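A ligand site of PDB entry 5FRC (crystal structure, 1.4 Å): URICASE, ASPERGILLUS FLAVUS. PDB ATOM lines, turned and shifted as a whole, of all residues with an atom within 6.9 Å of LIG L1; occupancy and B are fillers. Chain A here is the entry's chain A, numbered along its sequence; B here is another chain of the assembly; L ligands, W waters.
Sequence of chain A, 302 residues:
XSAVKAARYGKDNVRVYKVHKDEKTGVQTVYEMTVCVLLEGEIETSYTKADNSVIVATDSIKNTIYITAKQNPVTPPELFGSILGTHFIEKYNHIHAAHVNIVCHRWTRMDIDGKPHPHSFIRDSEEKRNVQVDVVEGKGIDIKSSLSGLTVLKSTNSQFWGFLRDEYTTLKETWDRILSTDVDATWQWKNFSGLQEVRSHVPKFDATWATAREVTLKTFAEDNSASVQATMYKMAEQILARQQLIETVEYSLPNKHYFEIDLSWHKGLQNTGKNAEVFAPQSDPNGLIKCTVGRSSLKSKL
The side-chain amide nitrogen (ND2) of Asn 255 sits close to a nitrogen (N2) of LIG L1 (3.4 Å). The backbone NH of Val 228 sits at hydrogen-bond distance from an oxygen (O1) of LIG L1 (2.9 Å). N of Thr 58 of chain B is in hydrogen-bond range of N3 of LIG L1, at 2.8 Å. The side-chain amide nitrogen (ND2) of Asn 255 sits at hydrogen-bond distance from an oxygen (O2) of LG2 L2 (2.9 Å). The side-chain hydroxyl of Thr 58 of chain B lies within hydrogen-bond range of a nitrogen (N3) of LIG L1 (3.2 Å). O1 of LIG L1 is in hydrogen-bond range of NH2 of Arg 177 (2.8 Å). O1 of LG2 L2 sits at hydrogen-bond distance from OG1 of Thr 58 of chain B, 2.6 Å away. An oxygen (O2) of LIG L1 sits at hydrogen-bond distance from the side-chain amide nitrogen (NE2) of Gln 229.
N2 of LIG L1 lies close to O2 of LG2 L2, at 3.4 Å.
O of Gly 287 lies within hydrogen-bond range of N of Asn 255 (2.8 Å). The backbone carbonyl oxygen (O) of Ser 227 sits at hydrogen-bond distance from the side-chain hydroxyl (OG) of Ser 225, at 2.9 Å. The side-chain amino group (NZ) of Lys 11 of chain B lies within hydrogen-bond range of the side-chain hydroxyl (OG1) of Thr 58 of chain B (2.8 Å). N of Ala 230 sits at hydrogen-bond distance from OG of Ser 227 (2.9 Å). The backbone carbonyl oxygen of Asn 255 lies within hydrogen-bond range of a ring nitrogen (NE2) of His 257 (3.3 Å). The backbone NH of Arg 177 sits at hydrogen-bond distance from the backbone carbonyl oxygen of Ser 158, 2.9 Å away. The backbone NH (N) of Gln 229 lies close to the side-chain hydroxyl (OG) of Ser 227 (3.3 Å). The side-chain hydroxyl (OH) of Tyr 9 of chain B sits at hydrogen-bond distance from the backbone carbonyl oxygen (O) of Val 56 of chain B, at 2.6 Å.
Phe 160 touches LIG L1 (CE2 to C2, 3.3 Å). CD2 of Leu 171 touches N4 of LIG L1, at 3.7 Å. Ser 227 touches LIG L1. CD1 of Ile 289 touches O2 of LIG L1, at 3.98 Å. Tyr 9 of chain B touches LIG L1 (CD2 to O2, 3.9 Å). CG2 of Ile 55 of chain B touches O2 of LIG L1, 3.4 Å away. CA of Ala 57 of chain B touches N3 of LIG L1, at 3.5 Å. Asp 59 of chain B touches LIG L1 (N to N4, 3.7 Å). Hydrophobic or aromatic side chains that line LIG L1: Phe 160, Leu 171, Val 228, Ile 289, Tyr 9 of chain B, Ile 55 of chain B and Ala 57 of chain B. Within 4 Å of LIG L1: Phe 160, Leu 171, Arg 177, Ser 227, Val 228, Gln 229, Asn 255, Ile 289, Tyr 9 of chain B, Ile 55 of chain B, Ala 57 of chain B, Thr 58 of chain B and Asp 59 of chain B.
Water W1 bridges N5 of LIG L1 (2.8 Å) and NH1 of Arg 177 (3.5 Å).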
ATOM      1  N   SER A 158       2.090  38.543  -2.283  1.00  0.00           N
ATOM      2  CA  SER A 158       1.893  37.253  -1.645  1.00  0.00           C
ATOM      3  C   SER A 158       2.155  37.454  -0.156  1.00  0.00           C
ATOM      4  O   SER A 158       3.113  38.140   0.233  1.00  0.00           O
ATOM      5  CB  SER A 158       2.824  36.197  -2.242  1.00  0.00           C
ATOM      6  OG  SER A 158       2.785  35.002  -1.480  1.00  0.00           O
ATOM      7  N   GLN A 159       1.282  36.888   0.666  1.00  0.00           N
ATOM      8  CA  GLN A 159       1.360  37.028   2.119  1.00  0.00           C
ATOM      9  C   GLN A 159       1.271  35.653   2.765  1.00  0.00           C
ATOM     10  O   GLN A 159       0.772  34.703   2.150  1.00  0.00           O
ATOM     11  CB  GLN A 159       0.226  37.923   2.640  1.00  0.00           C
ATOM     12  CG  GLN A 159       0.078  39.237   1.881  1.00  0.00           C
ATOM     13  CD  GLN A 159      -0.909  40.188   2.517  1.00  0.00           C
ATOM     14  OE1 GLN A 159      -1.235  40.080   3.698  1.00  0.00           O
ATOM     15  NE2 GLN A 159      -1.398  41.133   1.727  1.00  0.00           N
ATOM     16  N   PHE A 160       1.754  35.527   4.000  1.00  0.00           N
ATOM     17  CA  PHE A 160       1.479  34.340   4.783  1.00  0.00           C
ATOM     18  C   PHE A 160       1.622  34.659   6.267  1.00  0.00           C
ATOM     19  O   PHE A 160       2.726  34.723   6.813  1.00  0.00           O
ATOM     20  CB  PHE A 160       2.380  33.160   4.393  1.00  0.00           C
ATOM     21  CG  PHE A 160       1.944  31.850   4.985  1.00  0.00           C
ATOM     22  CD1 PHE A 160       0.676  31.346   4.702  1.00  0.00           C
ATOM     23  CD2 PHE A 160       2.775  31.130   5.829  1.00  0.00           C
ATOM     24  CE1 PHE A 160       0.252  30.142   5.260  1.00  0.00           C
ATOM     25  CE2 PHE A 160       2.360  29.930   6.383  1.00  0.00           C
ATOM     26  CZ  PHE A 160       1.100  29.429   6.096  1.00  0.00           C
ATOM     27  N   PHE A 163      -0.820  31.737  10.709  1.00  0.00           N
ATOM     28  CA  PHE A 163      -0.694  30.291  10.823  1.00  0.00           C
ATOM     29  C   PHE A 163      -0.419  29.859  12.261  1.00  0.00           C
ATOM     30  O   PHE A 163      -0.061  30.693  13.101  1.00  0.00           O
ATOM     31  CB  PHE A 163       0.389  29.766   9.882  1.00  0.00           C
ATOM     32  CG  PHE A 163       1.703  30.490  10.014  1.00  0.00           C
ATOM     33  CD1 PHE A 163       2.665  30.061  10.914  1.00  0.00           C
ATOM     34  CD2 PHE A 163       1.984  31.592   9.215  1.00  0.00           C
ATOM     35  CE1 PHE A 163       3.881  30.718  11.018  1.00  0.00           C
ATOM     36  CE2 PHE A 163       3.196  32.256   9.314  1.00  0.00           C
ATOM     37  CZ  PHE A 163       4.140  31.820  10.221  1.00  0.00           C
ATOM     38  N   LEU A 171       9.053  30.086  11.740  1.00  0.00           N
ATOM     39  CA  LEU A 171       8.709  30.921  10.585  1.00  0.00           C
ATOM     40  C   LEU A 171       8.071  32.229  11.018  1.00  0.00           C
ATOM     41  O   LEU A 171       7.090  32.237  11.761  1.00  0.00           O
ATOM     42  CB  LEU A 171       7.749  30.179   9.655  1.00  0.00           C
ATOM     43  CG  LEU A 171       7.351  30.913   8.368  1.00  0.00           C
ATOM     44  CD1 LEU A 171       8.582  31.143   7.487  1.00  0.00           C
ATOM     45  CD2 LEU A 171       6.278  30.137   7.616  1.00  0.00           C
ATOM     46  N   ARG A 177       5.963  38.686   0.372  1.00  0.00           N
ATOM     47  CA  ARG A 177       6.974  37.696   0.025  1.00  0.00           C
ATOM     48  C   ARG A 177       6.904  37.374  -1.453  1.00  0.00           C
ATOM     49  O   ARG A 177       5.935  37.709  -2.146  1.00  0.00           O
ATOM     50  CB  ARG A 177       6.787  36.416   0.847  1.00  0.00           C
ATOM     51  CG  ARG A 177       5.516  35.651   0.485  1.00  0.00           C
ATOM     52  CD  ARG A 177       5.336  34.352   1.246  1.00  0.00           C
ATOM     53  NE  ARG A 177       4.153  33.649   0.760  1.00  0.00           N
ATOM     54  CZ  ARG A 177       3.783  32.434   1.150  1.00  0.00           C
ATOM     55  NH1 ARG A 177       4.493  31.777   2.074  1.00  0.00           N
ATOM     56  NH2 ARG A 177       2.722  31.859   0.613  1.00  0.00           N
ATOM     57  N   LEU A 179       6.343  34.612  -4.318  1.00  0.00           N
ATOM     58  CA  LEU A 179       5.670  33.333  -4.515  1.00  0.00           C
ATOM     59  C   LEU A 179       6.031  32.769  -5.881  1.00  0.00           C
ATOM     60  O   LEU A 179       5.814  33.414  -6.912  1.00  0.00           O
ATOM     61  CB  LEU A 179       4.157  33.476  -4.381  1.00  0.00           C
ATOM     62  CG  LEU A 179       3.363  32.184  -4.580  1.00  0.00           C
ATOM     63  CD1 LEU A 179       3.821  31.110  -3.593  1.00  0.00           C
ATOM     64  CD2 LEU A 179       1.873  32.453  -4.460  1.00  0.00           C
ATOM     65  N   SER A 225      -2.311  37.105  -2.513  1.00  0.00           N
ATOM     66  CA  SER A 225      -2.452  35.749  -1.982  1.00  0.00           C
ATOM     67  C   SER A 225      -2.300  35.631  -0.463  1.00  0.00           C
ATOM     68  O   SER A 225      -1.314  36.082   0.104  1.00  0.00           O
ATOM     69  CB  SER A 225      -1.439  34.851  -2.669  1.00  0.00           C
ATOM     70  OG  SER A 225      -1.441  33.550  -2.106  1.00  0.00           O
ATOM     71  N   ALA A 226      -3.285  35.013   0.190  1.00  0.00           N
ATOM     72  CA  ALA A 226      -3.254  34.758   1.634  1.00  0.00           C
ATOM     73  C   ALA A 226      -2.434  33.527   1.962  1.00  0.00           C
ATOM     74  O   ALA A 226      -1.962  33.359   3.093  1.00  0.00           O
ATOM     75  CB  ALA A 226      -4.662  34.613   2.176  1.00  0.00           C
ATOM     76  N   SER A 227      -2.284  32.647   0.962  1.00  0.00           N
ATOM     77  CA  SER A 227      -1.576  31.376   1.076  1.00  0.00           C
ATOM     78  C   SER A 227      -1.652  30.710  -0.281  1.00  0.00           C
ATOM     79  O   SER A 227      -2.495  31.084  -1.111  1.00  0.00           O
ATOM     80  CB  SER A 227      -2.201  30.462   2.138  1.00  0.00           C
ATOM     81  OG  SER A 227      -3.486  30.063   1.715  1.00  0.00           O
ATOM     82  N   VAL A 228      -0.813  29.718  -0.512  1.00  0.00           N
ATOM     83  CA  VAL A 228      -0.940  28.893  -1.723  1.00  0.00           C
ATOM     84  C   VAL A 228      -2.326  28.210  -1.730  1.00  0.00           C
ATOM     85  O   VAL A 228      -2.995  28.162  -2.768  1.00  0.00           O
ATOM     86  CB  VAL A 228       0.182  27.846  -1.815  1.00  0.00           C
ATOM     87  CG1 VAL A 228      -0.017  26.952  -3.020  1.00  0.00           C
ATOM     88  CG2 VAL A 228       1.554  28.542  -1.949  1.00  0.00           C
ATOM     89  N   GLN A 229      -2.731  27.728  -0.557  1.00  0.00           N
ATOM     90  CA  GLN A 229      -4.027  27.075  -0.388  1.00  0.00           C
ATOM     91  C   GLN A 229      -5.172  27.948  -0.900  1.00  0.00           C
ATOM     92  O   GLN A 229      -6.035  27.485  -1.666  1.00  0.00           O
ATOM     93  CB  GLN A 229      -4.277  26.732   1.097  1.00  0.00           C
ATOM     94  CG  GLN A 229      -3.444  25.586   1.668  1.00  0.00           C
ATOM     95  CD  GLN A 229      -2.063  26.015   2.194  1.00  0.00           C
ATOM     96  OE1 GLN A 229      -1.493  27.018   1.766  1.00  0.00           O
ATOM     97  NE2 GLN A 229      -1.525  25.227   3.127  1.00  0.00           N
ATOM     98  N   ALA A 230      -5.195  29.211  -0.470  1.00  0.00           N
ATOM     99  CA  ALA A 230      -6.319  30.089  -0.772  1.00  0.00           C
ATOM    100  C   ALA A 230      -6.339  30.450  -2.250  1.00  0.00           C
ATOM    101  O   ALA A 230      -7.398  30.544  -2.870  1.00  0.00           O
ATOM    102  CB  ALA A 230      -6.255  31.339   0.079  1.00  0.00           C
ATOM    103  N   ASN A 255       5.736  25.163  -3.222  1.00  0.00           N
ATOM    104  CA  ASN A 255       6.099  26.521  -2.850  1.00  0.00           C
ATOM    105  C   ASN A 255       7.613  26.593  -2.958  1.00  0.00           C
ATOM    106  O   ASN A 255       8.313  26.061  -2.104  1.00  0.00           O
ATOM    107  CB  ASN A 255       5.613  26.843  -1.442  1.00  0.00           C
ATOM    108  CG  ASN A 255       5.645  28.315  -1.121  1.00  0.00           C
ATOM    109  OD1 ASN A 255       6.278  29.103  -1.823  1.00  0.00           O
ATOM    110  ND2 ASN A 255       4.962  28.698  -0.069  1.00  0.00           N
ATOM    111  N   HIS A 257      10.720  28.192  -2.485  1.00  0.00           N
ATOM    112  CA  HIS A 257      11.038  29.307  -1.597  1.00  0.00           C
ATOM    113  C   HIS A 257      12.212  30.167  -2.070  1.00  0.00           C
ATOM    114  O   HIS A 257      13.206  29.655  -2.601  1.00  0.00           O
ATOM    115  CB  HIS A 257      11.357  28.790  -0.193  1.00  0.00           C
ATOM    116  CG  HIS A 257      10.291  27.897   0.374  1.00  0.00           C
ATOM    117  ND1 HIS A 257       9.038  28.356   0.716  1.00  0.00           N
ATOM    118  CD2 HIS A 257      10.305  26.569   0.652  1.00  0.00           C
ATOM    119  CE1 HIS A 257       8.315  27.343   1.180  1.00  0.00           C
ATOM    120  NE2 HIS A 257       9.065  26.250   1.146  1.00  0.00           N
ATOM    121  N   GLY A 287       7.614  23.600   0.174  1.00  0.00           N
ATOM    122  CA  GLY A 287       6.229  23.328   0.521  1.00  0.00           C
ATOM    123  C   GLY A 287       5.570  22.589  -0.639  1.00  0.00           C
ATOM    124  O   GLY A 287       5.931  22.795  -1.804  1.00  0.00           O
ATOM    125  N   ILE A 289       1.589  21.698  -1.725  1.00  0.00           N
ATOM    126  CA  ILE A 289       0.204  21.966  -1.363  1.00  0.00           C
ATOM    127  C   ILE A 289      -0.716  21.353  -2.408  1.00  0.00           C
ATOM    128  O   ILE A 289      -0.532  21.581  -3.592  1.00  0.00           O
ATOM    129  CB  ILE A 289      -0.071  23.486  -1.280  1.00  0.00           C
ATOM    130  CG1 ILE A 289       1.083  24.240  -0.607  1.00  0.00           C
ATOM    131  CG2 ILE A 289      -1.389  23.754  -0.539  1.00  0.00           C
ATOM    132  CD1 ILE A 289       1.342  23.878   0.834  1.00  0.00           C
ATOM    133  N   TYR B   9      -1.244  18.715   2.500  1.00  0.00           N
ATOM    134  CA  TYR B   9      -0.177  19.688   2.290  1.00  0.00           C
ATOM    135  C   TYR B   9       0.957  19.388   3.267  1.00  0.00           C
ATOM    136  O   TYR B   9       0.771  18.757   4.309  1.00  0.00           O
ATOM    137  CB  TYR B   9      -0.692  21.123   2.492  1.00  0.00           C
ATOM    138  CG  TYR B   9      -0.656  21.455   3.955  1.00  0.00           C
ATOM    139  CD1 TYR B   9      -1.603  20.928   4.833  1.00  0.00           C
ATOM    140  CD2 TYR B   9       0.381  22.223   4.487  1.00  0.00           C
ATOM    141  CE1 TYR B   9      -1.525  21.167   6.184  1.00  0.00           C
ATOM    142  CE2 TYR B   9       0.457  22.476   5.817  1.00  0.00           C
ATOM    143  CZ  TYR B   9      -0.489  21.949   6.671  1.00  0.00           C
ATOM    144  OH  TYR B   9      -0.398  22.179   8.015  1.00  0.00           O
ATOM    145  N   GLY B  10       2.156  19.875   2.967  1.00  0.00           N
ATOM    146  CA  GLY B  10       3.259  19.706   3.884  1.00  0.00           C
ATOM    147  C   GLY B  10       4.570  20.074   3.240  1.00  0.00           C
ATOM    148  O   GLY B  10       4.617  20.962   2.380  1.00  0.00           O
ATOM    149  N   LYS B  11       5.643  19.405   3.637  1.00  0.00           N
ATOM    150  CA  LYS B  11       6.981  19.726   3.130  1.00  0.00           C
ATOM    151  C   LYS B  11       7.545  18.533   2.389  1.00  0.00           C
ATOM    152  O   LYS B  11       7.545  17.406   2.908  1.00  0.00           O
ATOM    153  CB  LYS B  11       7.904  20.148   4.278  1.00  0.00           C
ATOM    154  CG  LYS B  11       9.169  20.897   3.832  1.00  0.00           C
ATOM    155  CD  LYS B  11       8.835  22.248   3.226  1.00  0.00           C
ATOM    156  CE  LYS B  11       9.317  23.408   4.078  1.00  0.00           C
ATOM    157  NZ  LYS B  11       8.722  24.703   3.658  1.00  0.00           N
ATOM    158  N   ASN B  52      -5.660  30.689   8.003  1.00  0.00           N
ATOM    159  CA  ASN B  52      -4.371  30.048   8.212  1.00  0.00           C
ATOM    160  C   ASN B  52      -4.193  29.476   9.609  1.00  0.00           C
ATOM    161  O   ASN B  52      -3.214  28.796   9.867  1.00  0.00           O
ATOM    162  CB  ASN B  52      -3.241  31.024   7.872  1.00  0.00           C
ATOM    163  CG  ASN B  52      -3.141  31.284   6.386  1.00  0.00           C
ATOM    164  OD1 ASN B  52      -3.541  30.443   5.579  1.00  0.00           O
ATOM    165  ND2 ASN B  52      -2.618  32.449   6.013  1.00  0.00           N
ATOM    166  N   ILE B  55      -3.361  25.861   9.734  1.00  0.00           N
ATOM    167  CA  ILE B  55      -2.150  25.393   9.065  1.00  0.00           C
ATOM    168  C   ILE B  55      -0.972  25.292  10.014  1.00  0.00           C
ATOM    169  O   ILE B  55      -0.529  26.290  10.592  1.00  0.00           O
ATOM    170  CB  ILE B  55      -1.766  26.314   7.893  1.00  0.00           C
ATOM    171  CG1 ILE B  55      -2.852  26.291   6.812  1.00  0.00           C
ATOM    172  CG2 ILE B  55      -0.427  25.874   7.289  1.00  0.00           C
ATOM    173  CD1 ILE B  55      -3.147  24.895   6.277  1.00  0.00           C
ATOM    174  N   VAL B  56      -0.477  24.068  10.192  1.00  0.00           N
ATOM    175  CA  VAL B  56       0.837  23.842  10.762  1.00  0.00           C
ATOM    176  C   VAL B  56       1.781  24.180   9.613  1.00  0.00           C
ATOM    177  O   VAL B  56       1.761  23.494   8.588  1.00  0.00           O
ATOM    178  CB  VAL B  56       1.003  22.386  11.240  1.00  0.00           C
ATOM    179  CG1 VAL B  56       2.416  22.133  11.769  1.00  0.00           C
ATOM    180  CG2 VAL B  56      -0.035  22.060  12.308  1.00  0.00           C
ATOM    181  N   ALA B  57       2.574  25.241   9.737  1.00  0.00           N
ATOM    182  CA  ALA B  57       3.364  25.713   8.600  1.00  0.00           C
ATOM    183  C   ALA B  57       4.254  24.607   8.053  1.00  0.00           C
ATOM    184  O   ALA B  57       4.788  23.812   8.823  1.00  0.00           O
ATOM    185  CB  ALA B  57       4.208  26.925   8.991  1.00  0.00           C
ATOM    186  N   THR B  58       4.398  24.555   6.734  1.00  0.00           N
ATOM    187  CA  THR B  58       5.286  23.559   6.151  1.00  0.00           C
ATOM    188  C   THR B  58       6.694  23.757   6.706  1.00  0.00           C
ATOM    189  O   THR B  58       7.407  22.788   6.920  1.00  0.00           O
ATOM    190  CB  THR B  58       5.308  23.609   4.596  1.00  0.00           C
ATOM    191  OG1 THR B  58       5.950  24.802   4.143  1.00  0.00           O
ATOM    192  CG2 THR B  58       3.878  23.573   4.069  1.00  0.00           C
ATOM    193  N   ASP B  59       7.078  25.003   6.981  1.00  0.00           N
ATOM    194  CA  ASP B  59       8.371  25.280   7.593  1.00  0.00           C
ATOM    195  C   ASP B  59       8.491  24.600   8.960  1.00  0.00           C
ATOM    196  O   ASP B  59       9.557  24.126   9.336  1.00  0.00           O
ATOM    197  CB  ASP B  59       8.588  26.782   7.741  1.00  0.00           C
ATOM    198  CG  ASP B  59       9.984  27.113   8.198  1.00  0.00           C
ATOM    199  OD1 ASP B  59      10.909  27.111   7.348  1.00  0.00           O
ATOM    200  OD2 ASP B  59      10.174  27.372   9.415  1.00  0.00           O
ATOM    201  N   SER B  60       7.389  24.571   9.705  1.00  0.00           N
ATOM    202  CA  SER B  60       7.358  23.912  11.001  1.00  0.00           C
ATOM    203  C   SER B  60       7.430  22.392  10.869  1.00  0.00           C
ATOM    204  O   SER B  60       8.032  21.721  11.706  1.00  0.00           O
ATOM    205  CB  SER B  60       6.088  24.304  11.763  1.00  0.00           C
ATOM    206  OG  SER B  60       6.039  25.713  11.954  1.00  0.00           O
HETATM  207  N1  LIG L   1       1.208  27.774   2.759  1.00  0.00           N
HETATM  208  C1  LIG L   1       1.894  28.835   2.279  1.00  0.00           C
HETATM  209  O1  LIG L   1       1.357  29.502   1.366  1.00  0.00           O
HETATM  210  N2  LIG L   1       3.116  29.203   2.742  1.00  0.00           N
HETATM  211  C2  LIG L   1       3.692  28.510   3.729  1.00  0.00           C
HETATM  212  C3  LIG L   1       2.983  27.351   4.312  1.00  0.00           C
HETATM  213  C4  LIG L   1       1.674  27.005   3.735  1.00  0.00           C
HETATM  214  O2  LIG L   1       1.029  26.025   4.169  1.00  0.00           O
HETATM  215  N3  LIG L   1       3.762  26.817   5.279  1.00  0.00           N
HETATM  216  N4  LIG L   1       4.926  27.592   5.346  1.00  0.00           N
HETATM  217  N5  LIG L   1       4.853  28.626   4.390  1.00  0.00           N
HETATM  218  O1  LG2 L   2       5.114  26.029   1.987  1.00  0.00           O
HETATM  219  O2  LG2 L   2       4.153  26.265   1.298  1.00  0.00           O
HETATM  220  O   HOH W   1       7.094  30.176   3.702  1.00  0.00           O
